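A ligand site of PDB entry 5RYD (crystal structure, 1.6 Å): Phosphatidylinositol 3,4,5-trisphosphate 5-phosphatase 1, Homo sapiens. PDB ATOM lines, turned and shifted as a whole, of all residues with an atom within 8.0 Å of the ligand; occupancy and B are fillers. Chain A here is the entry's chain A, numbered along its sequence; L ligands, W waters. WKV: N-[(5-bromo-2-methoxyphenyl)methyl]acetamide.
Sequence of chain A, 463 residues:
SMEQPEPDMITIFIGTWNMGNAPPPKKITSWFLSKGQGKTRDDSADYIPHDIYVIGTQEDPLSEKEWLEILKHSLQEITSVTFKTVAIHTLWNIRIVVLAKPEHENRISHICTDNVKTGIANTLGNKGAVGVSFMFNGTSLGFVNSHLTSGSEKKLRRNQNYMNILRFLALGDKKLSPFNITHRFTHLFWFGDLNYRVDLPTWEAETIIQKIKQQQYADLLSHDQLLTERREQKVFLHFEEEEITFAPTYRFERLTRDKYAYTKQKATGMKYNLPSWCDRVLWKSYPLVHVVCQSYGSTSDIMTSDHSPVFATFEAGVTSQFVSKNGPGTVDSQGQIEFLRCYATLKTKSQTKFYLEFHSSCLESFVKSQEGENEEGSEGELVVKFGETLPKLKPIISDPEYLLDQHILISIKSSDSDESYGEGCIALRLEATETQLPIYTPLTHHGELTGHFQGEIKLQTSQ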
ATOM      1  N   LEU A  68      -0.226  17.933   1.371  1.00  0.00           N
ATOM      2  CA  LEU A  68       0.918  17.192   0.789  1.00  0.00           C
ATOM      3  C   LEU A  68       2.170  17.338   1.654  1.00  0.00           C
ATOM      4  O   LEU A  68       2.874  16.347   1.879  1.00  0.00           O
ATOM      5  CB  LEU A  68       1.171  17.619  -0.648  1.00  0.00           C
ATOM      6  CG  LEU A  68       0.176  17.053  -1.636  1.00  0.00           C
ATOM      7  CD1 LEU A  68       0.240  17.773  -2.962  1.00  0.00           C
ATOM      8  CD2 LEU A  68       0.402  15.559  -1.814  1.00  0.00           C
ATOM      9  N   LYS A  72       3.651  13.978   3.258  1.00  0.00           N
ATOM     10  CA  LYS A  72       4.993  13.523   2.807  1.00  0.00           C
ATOM     11  C   LYS A  72       6.008  13.523   3.969  1.00  0.00           C
ATOM     12  O   LYS A  72       6.743  12.527   4.128  1.00  0.00           O
ATOM     13  CB  LYS A  72       5.501  14.340   1.637  1.00  0.00           C
ATOM     14  CG  LYS A  72       4.728  14.074   0.368  1.00  0.00           C
ATOM     15  CD  LYS A  72       5.586  14.298  -0.838  1.00  0.00           C
ATOM     16  CE  LYS A  72       5.034  13.525  -1.983  1.00  0.00           C
ATOM     17  NZ  LYS A  72       5.784  13.810  -3.218  1.00  0.00           N
ATOM     18  N   PHE A  83       8.200   9.876  -0.504  1.00  0.00           N
ATOM     19  CA  PHE A  83       7.135   9.287  -1.354  1.00  0.00           C
ATOM     20  C   PHE A  83       6.893  10.178  -2.567  1.00  0.00           C
ATOM     21  O   PHE A  83       6.953  11.382  -2.481  1.00  0.00           O
ATOM     22  CB  PHE A  83       5.890   9.067  -0.489  1.00  0.00           C
ATOM     23  CG  PHE A  83       5.958   7.743   0.223  1.00  0.00           C
ATOM     24  CD1 PHE A  83       6.746   7.599   1.338  1.00  0.00           C
ATOM     25  CD2 PHE A  83       5.326   6.632  -0.307  1.00  0.00           C
ATOM     26  CE1 PHE A  83       6.884   6.358   1.944  1.00  0.00           C
ATOM     27  CE2 PHE A  83       5.459   5.399   0.305  1.00  0.00           C
ATOM     28  CZ  PHE A  83       6.219   5.264   1.441  1.00  0.00           C
ATOM     29  N   LYS A  84       6.580   9.571  -3.688  1.00  0.00           N
ATOM     30  CA  LYS A  84       6.164  10.300  -4.911  1.00  0.00           C
ATOM     31  C   LYS A  84       4.661  10.517  -4.880  1.00  0.00           C
ATOM     32  O   LYS A  84       3.945   9.591  -4.433  1.00  0.00           O
ATOM     33  CB  LYS A  84       6.495   9.484  -6.146  1.00  0.00           C
ATOM     34  CG  LYS A  84       7.985   9.257  -6.340  1.00  0.00           C
ATOM     35  CD  LYS A  84       8.711  10.443  -6.891  1.00  0.00           C
ATOM     36  CE  LYS A  84      10.164  10.142  -7.107  1.00  0.00           C
ATOM     37  NZ  LYS A  84      10.864  11.360  -7.567  1.00  0.00           N
ATOM     38  N   THR A  85       4.205  11.642  -5.434  1.00  0.00           N
ATOM     39  CA  THR A  85       2.755  11.954  -5.522  1.00  0.00           C
ATOM     40  C   THR A  85       2.223  11.366  -6.812  1.00  0.00           C
ATOM     41  O   THR A  85       2.685  11.772  -7.861  1.00  0.00           O
ATOM     42  CB  THR A  85       2.506  13.466  -5.435  1.00  0.00           C
ATOM     43  OG1 THR A  85       3.105  13.967  -4.238  1.00  0.00           O
ATOM     44  CG2 THR A  85       1.036  13.785  -5.470  1.00  0.00           C
ATOM     45  N   VAL A  86       1.310  10.410  -6.726  1.00  0.00           N
ATOM     46  CA  VAL A  86       0.669   9.815  -7.920  1.00  0.00           C
ATOM     47  C   VAL A  86      -0.431  10.743  -8.372  1.00  0.00           C
ATOM     48  O   VAL A  86      -0.522  11.071  -9.604  1.00  0.00           O
ATOM     49  CB  VAL A  86       0.107   8.423  -7.579  1.00  0.00           C
ATOM     50  CG1 VAL A  86      -0.688   7.855  -8.730  1.00  0.00           C
ATOM     51  CG2 VAL A  86       1.234   7.496  -7.165  1.00  0.00           C
ATOM     52  N   ALA A  87      -1.295  11.123  -7.448  1.00  0.00           N
ATOM     53  CA  ALA A  87      -2.462  11.959  -7.777  1.00  0.00           C
ATOM     54  C   ALA A  87      -2.988  12.645  -6.520  1.00  0.00           C
ATOM     55  O   ALA A  87      -2.814  12.158  -5.399  1.00  0.00           O
ATOM     56  CB  ALA A  87      -3.517  11.097  -8.442  1.00  0.00           C
ATOM     57  N   ILE A  88      -3.644  13.776  -6.713  1.00  0.00           N
ATOM     58  CA  ILE A  88      -4.401  14.465  -5.654  1.00  0.00           C
ATOM     59  C   ILE A  88      -5.632  15.061  -6.330  1.00  0.00           C
ATOM     60  O   ILE A  88      -5.499  15.571  -7.471  1.00  0.00           O
ATOM     61  CB  ILE A  88      -3.523  15.473  -4.902  1.00  0.00           C
ATOM     62  CG1 ILE A  88      -4.328  16.140  -3.812  1.00  0.00           C
ATOM     63  CG2 ILE A  88      -2.850  16.486  -5.812  1.00  0.00           C
ATOM     64  CD1 ILE A  88      -3.436  16.839  -2.837  1.00  0.00           C
ATOM     65  N   VAL A  98      -2.929  10.148  -3.379  1.00  0.00           N
ATOM     66  CA  VAL A  98      -2.268   8.853  -3.608  1.00  0.00           C
ATOM     67  C   VAL A  98      -0.757   9.077  -3.656  1.00  0.00           C
ATOM     68  O   VAL A  98      -0.300   9.879  -4.480  1.00  0.00           O
ATOM     69  CB  VAL A  98      -2.764   8.146  -4.865  1.00  0.00           C
ATOM     70  CG1 VAL A  98      -1.996   6.835  -5.054  1.00  0.00           C
ATOM     71  CG2 VAL A  98      -4.256   7.906  -4.795  1.00  0.00           C
ATOM     72  N   LEU A  99      -0.049   8.413  -2.738  1.00  0.00           N
ATOM     73  CA  LEU A  99       1.425   8.449  -2.674  1.00  0.00           C
ATOM     74  C   LEU A  99       1.980   7.052  -2.905  1.00  0.00           C
ATOM     75  O   LEU A  99       1.397   6.071  -2.477  1.00  0.00           O
ATOM     76  CB  LEU A  99       1.868   8.975  -1.309  1.00  0.00           C
ATOM     77  CG  LEU A  99       1.225  10.278  -0.849  1.00  0.00           C
ATOM     78  CD1 LEU A  99       1.743  10.662   0.518  1.00  0.00           C
ATOM     79  CD2 LEU A  99       1.479  11.412  -1.836  1.00  0.00           C
ATOM     80  N   ALA A 100       3.160   6.975  -3.492  1.00  0.00           N
ATOM     81  CA  ALA A 100       3.783   5.677  -3.773  1.00  0.00           C
ATOM     82  C   ALA A 100       5.287   5.726  -3.535  1.00  0.00           C
ATOM     83  O   ALA A 100       5.880   6.765  -3.692  1.00  0.00           O
ATOM     84  CB  ALA A 100       3.508   5.295  -5.206  1.00  0.00           C
ATOM     85  N   LYS A 101       5.869   4.591  -3.158  1.00  0.00           N
ATOM     86  CA  LYS A 101       7.335   4.472  -3.004  1.00  0.00           C
ATOM     87  C   LYS A 101       7.990   4.827  -4.333  1.00  0.00           C
ATOM     88  O   LYS A 101       7.452   4.482  -5.388  1.00  0.00           O
ATOM     89  CB  LYS A 101       7.712   3.048  -2.573  1.00  0.00           C
ATOM     90  CG  LYS A 101       7.080   2.609  -1.258  1.00  0.00           C
ATOM     91  CD  LYS A 101       7.588   1.259  -0.823  1.00  0.00           C
ATOM     92  CE  LYS A 101       9.097   1.209  -0.673  1.00  0.00           C
ATOM     93  NZ  LYS A 101       9.578  -0.193  -0.594  1.00  0.00           N
ATOM     94  N   PRO A 102       9.138   5.534  -4.332  1.00  0.00           N
ATOM     95  CA  PRO A 102       9.805   5.933  -5.571  1.00  0.00           C
ATOM     96  C   PRO A 102      10.107   4.772  -6.526  1.00  0.00           C
ATOM     97  O   PRO A 102      10.013   4.971  -7.724  1.00  0.00           O
ATOM     98  CB  PRO A 102      11.099   6.599  -5.124  1.00  0.00           C
ATOM     99  CG  PRO A 102      11.136   6.537  -3.634  1.00  0.00           C
ATOM    100  CD  PRO A 102       9.830   5.983  -3.111  1.00  0.00           C
ATOM    101  N   HIS A 104       8.241   2.560  -7.392  1.00  0.00           N
ATOM    102  CA  HIS A 104       7.013   2.239  -8.149  1.00  0.00           C
ATOM    103  C   HIS A 104       6.674   3.263  -9.203  1.00  0.00           C
ATOM    104  O   HIS A 104       5.738   3.012  -9.964  1.00  0.00           O
ATOM    105  CB  HIS A 104       5.838   2.068  -7.213  1.00  0.00           C
ATOM    106  CG  HIS A 104       6.037   0.925  -6.288  1.00  0.00           C
ATOM    107  ND1 HIS A 104       6.704  -0.243  -6.669  1.00  0.00           N
ATOM    108  CD2 HIS A 104       5.642   0.756  -5.009  1.00  0.00           C
ATOM    109  CE1 HIS A 104       6.667  -1.085  -5.644  1.00  0.00           C
ATOM    110  NE2 HIS A 104       6.041  -0.487  -4.612  1.00  0.00           N
ATOM    111  N   GLU A 105       7.439   4.350  -9.297  1.00  0.00           N
ATOM    112  CA  GLU A 105       7.100   5.455 -10.228  1.00  0.00           C
ATOM    113  C   GLU A 105       6.836   4.946 -11.662  1.00  0.00           C
ATOM    114  O   GLU A 105       5.840   5.345 -12.291  1.00  0.00           O
ATOM    115  CB  GLU A 105       8.166   6.547 -10.177  1.00  0.00           C
ATOM    116  CG  GLU A 105       7.967   7.566 -11.260  1.00  0.00           C
ATOM    117  CD  GLU A 105       8.915   8.753 -11.217  1.00  0.00           C
ATOM    118  OE1 GLU A 105       9.662   8.808 -10.264  1.00  0.00           O
ATOM    119  OE2 GLU A 105       8.896   9.597 -12.151  1.00  0.00           O
ATOM    120  N   ASN A 106       7.703   4.068 -12.163  1.00  0.00           N
ATOM    121  CA  ASN A 106       7.655   3.598 -13.581  1.00  0.00           C
ATOM    122  C   ASN A 106       6.783   2.348 -13.705  1.00  0.00           C
ATOM    123  O   ASN A 106       6.671   1.833 -14.825  1.00  0.00           O
ATOM    124  CB  ASN A 106       9.076   3.464 -14.127  1.00  0.00           C
ATOM    125  CG  ASN A 106       9.723   4.825 -14.259  1.00  0.00           C
ATOM    126  OD1 ASN A 106       9.397   5.580 -15.173  1.00  0.00           O
ATOM    127  ND2 ASN A 106      10.594   5.164 -13.324  1.00  0.00           N
ATOM    128  N   ARG A 107       6.159   1.894 -12.607  1.00  0.00           N
ATOM    129  CA  ARG A 107       5.160   0.775 -12.616  1.00  0.00           C
ATOM    130  C   ARG A 107       3.752   1.360 -12.737  1.00  0.00           C
ATOM    131  O   ARG A 107       2.819   0.638 -13.096  1.00  0.00           O
ATOM    132  CB  ARG A 107       5.274  -0.075 -11.358  1.00  0.00           C
ATOM    133  CG  ARG A 107       6.617  -0.771 -11.249  1.00  0.00           C
ATOM    134  CD  ARG A 107       6.657  -1.629 -10.005  1.00  0.00           C
ATOM    135  NE  ARG A 107       7.851  -2.435 -10.090  1.00  0.00           N
ATOM    136  CZ  ARG A 107       8.790  -2.564  -9.190  1.00  0.00           C
ATOM    137  NH1 ARG A 107       8.738  -1.915  -8.039  1.00  0.00           N
ATOM    138  NH2 ARG A 107       9.809  -3.347  -9.450  1.00  0.00           N
ATOM    139  N   ILE A 108       3.625   2.662 -12.543  1.00  0.00           N
ATOM    140  CA  ILE A 108       2.305   3.333 -12.427  1.00  0.00           C
ATOM    141  C   ILE A 108       2.004   4.115 -13.711  1.00  0.00           C
ATOM    142  O   ILE A 108       2.849   4.883 -14.163  1.00  0.00           O
ATOM    143  CB  ILE A 108       2.256   4.211 -11.152  1.00  0.00           C
ATOM    144  CG1 ILE A 108       2.266   3.321  -9.908  1.00  0.00           C
ATOM    145  CG2 ILE A 108       1.063   5.164 -11.172  1.00  0.00           C
ATOM    146  CD1 ILE A 108       2.616   4.066  -8.639  1.00  0.00           C
ATOM    147  N   SER A 109       0.803   3.954 -14.237  1.00  0.00           N
ATOM    148  CA  SER A 109       0.375   4.587 -15.509  1.00  0.00           C
ATOM    149  C   SER A 109      -1.138   4.726 -15.530  1.00  0.00           C
ATOM    150  O   SER A 109      -1.825   4.253 -14.603  1.00  0.00           O
ATOM    151  CB  SER A 109       0.887   3.791 -16.731  1.00  0.00           C
ATOM    152  OG  SER A 109       0.127   2.594 -16.894  1.00  0.00           O
ATOM    153  N   HIS A 110      -1.652   5.367 -16.564  1.00  0.00           N
ATOM    154  CA  HIS A 110      -3.121   5.505 -16.789  1.00  0.00           C
ATOM    155  C   HIS A 110      -3.790   6.079 -15.555  1.00  0.00           C
ATOM    156  O   HIS A 110      -4.821   5.559 -15.120  1.00  0.00           O
ATOM    157  CB  HIS A 110      -3.727   4.173 -17.201  1.00  0.00           C
ATOM    158  CG  HIS A 110      -3.181   3.673 -18.500  1.00  0.00           C
ATOM    159  ND1 HIS A 110      -2.006   2.983 -18.554  1.00  0.00           N
ATOM    160  CD2 HIS A 110      -3.623   3.792 -19.771  1.00  0.00           C
ATOM    161  CE1 HIS A 110      -1.773   2.638 -19.805  1.00  0.00           C
ATOM    162  NE2 HIS A 110      -2.727   3.132 -20.563  1.00  0.00           N
ATOM    163  N   ILE A 111      -3.234   7.154 -14.996  1.00  0.00           N
ATOM    164  CA  ILE A 111      -3.812   7.779 -13.797  1.00  0.00           C
ATOM    165  C   ILE A 111      -5.054   8.539 -14.222  1.00  0.00           C
ATOM    166  O   ILE A 111      -5.006   9.329 -15.197  1.00  0.00           O
ATOM    167  CB  ILE A 111      -2.792   8.677 -13.095  1.00  0.00           C
ATOM    168  CG1 ILE A 111      -1.557   7.887 -12.672  1.00  0.00           C
ATOM    169  CG2 ILE A 111      -3.395   9.442 -11.930  1.00  0.00           C
ATOM    170  CD1 ILE A 111      -0.365   8.750 -12.458  1.00  0.00           C
ATOM    171  N   PHE A 134      -5.505   3.911 -11.422  1.00  0.00           N
ATOM    172  CA  PHE A 134      -4.287   3.784 -12.228  1.00  0.00           C
ATOM    173  C   PHE A 134      -3.993   2.318 -12.426  1.00  0.00           C
ATOM    174  O   PHE A 134      -4.592   1.493 -11.761  1.00  0.00           O
ATOM    175  CB  PHE A 134      -3.118   4.515 -11.562  1.00  0.00           C
ATOM    176  CG  PHE A 134      -2.834   4.147 -10.132  1.00  0.00           C
ATOM    177  CD1 PHE A 134      -3.455   4.792  -9.064  1.00  0.00           C
ATOM    178  CD2 PHE A 134      -1.913   3.142  -9.850  1.00  0.00           C
ATOM    179  CE1 PHE A 134      -3.114   4.470  -7.758  1.00  0.00           C
ATOM    180  CE2 PHE A 134      -1.574   2.825  -8.552  1.00  0.00           C
ATOM    181  CZ  PHE A 134      -2.200   3.504  -7.500  1.00  0.00           C
ATOM    182  N   MET A 135      -3.036   2.050 -13.294  1.00  0.00           N
ATOM    183  CA  MET A 135      -2.476   0.705 -13.498  1.00  0.00           C
ATOM    184  C   MET A 135      -1.207   0.614 -12.683  1.00  0.00           C
ATOM    185  O   MET A 135      -0.397   1.578 -12.689  1.00  0.00           O
ATOM    186  CB  MET A 135      -2.129   0.468 -14.976  1.00  0.00           C
ATOM    187  CG  MET A 135      -3.333   0.344 -15.872  1.00  0.00           C
ATOM    188  SD  MET A 135      -4.399  -1.076 -15.559  1.00  0.00           S
ATOM    189  CE  MET A 135      -3.252  -2.424 -15.835  1.00  0.00           C
HETATM  190  C10 WKV L   1       1.914  11.728 -12.357  1.00  0.00           C
HETATM  191  C01 WKV L   1       2.484   9.120 -15.542  1.00  0.00           C
HETATM  192  C03 WKV L   1       2.794   9.556 -13.190  1.00  0.00           C
HETATM  193  C04 WKV L   1       3.443   8.330 -13.001  1.00  0.00           C
HETATM  194  C05 WKV L   1       3.927   7.986 -11.755  1.00  0.00           C
HETATM  195  C06 WKV L   1       3.773   8.844 -10.691  1.00  0.00           C
HETATM  196  C08 WKV L   1       3.132  10.068 -10.848  1.00  0.00           C
HETATM  197  C09 WKV L   1       2.646  10.421 -12.112  1.00  0.00           C
HETATM  198  C12 WKV L   1       2.118  13.757 -10.842  1.00  0.00           C
HETATM  199  C14 WKV L   1       1.793  14.461  -9.531  1.00  0.00           C
HETATM  200  N11 WKV L   1       1.610  12.425 -11.100  1.00  0.00           N
HETATM  201  O02 WKV L   1       2.297   9.968 -14.431  1.00  0.00           O
HETATM  202  O13 WKV L   1       2.791  14.299 -11.660  1.00  0.00           O
HETATM  203 BR7  WKV L   1       4.487   8.316  -8.988  1.00  0.00          BR
HETATM  204  O   HOH W   1       0.909   7.254 -17.688  1.00  0.00           O
HETATM  205  O   HOH W   2      -0.511  11.234 -15.578  1.00  0.00           O
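The backbone carbonyl oxygen (O) of Val 86 lies within hydrogen-bond range of a nitrogen (N11) of the ligand.
N11 of the ligand sits close to O of Thr 85, 3.5 Å away.
NZ of Lys 84 is in salt-bridge range of OE1 of Glu 105 (3.9 Å).
The backbone carbonyl oxygen (O) of Lys 84 sits at hydrogen-bond distance from the backbone NH (N) of Ala 100, 2.9 Å away.
The backbone NH (N) of Val 86 is in hydrogen-bond range of the backbone carbonyl oxygen (O) of Val 98 (2.8 Å).
NZ of Lys 72 lies within hydrogen-bond range of OG1 of Thr 85 (2.9 Å).
Merely in contact with the ligand: Glu 105, Ile 111, Lys 84 and Ile 108.
Within 4 Å of the ligand: Lys 84, Thr 85, Val 86, Glu 105, Ile 108 and Ile 111.
Along chain A the residues within 4 Å of the ligand span positions 84 to 111.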
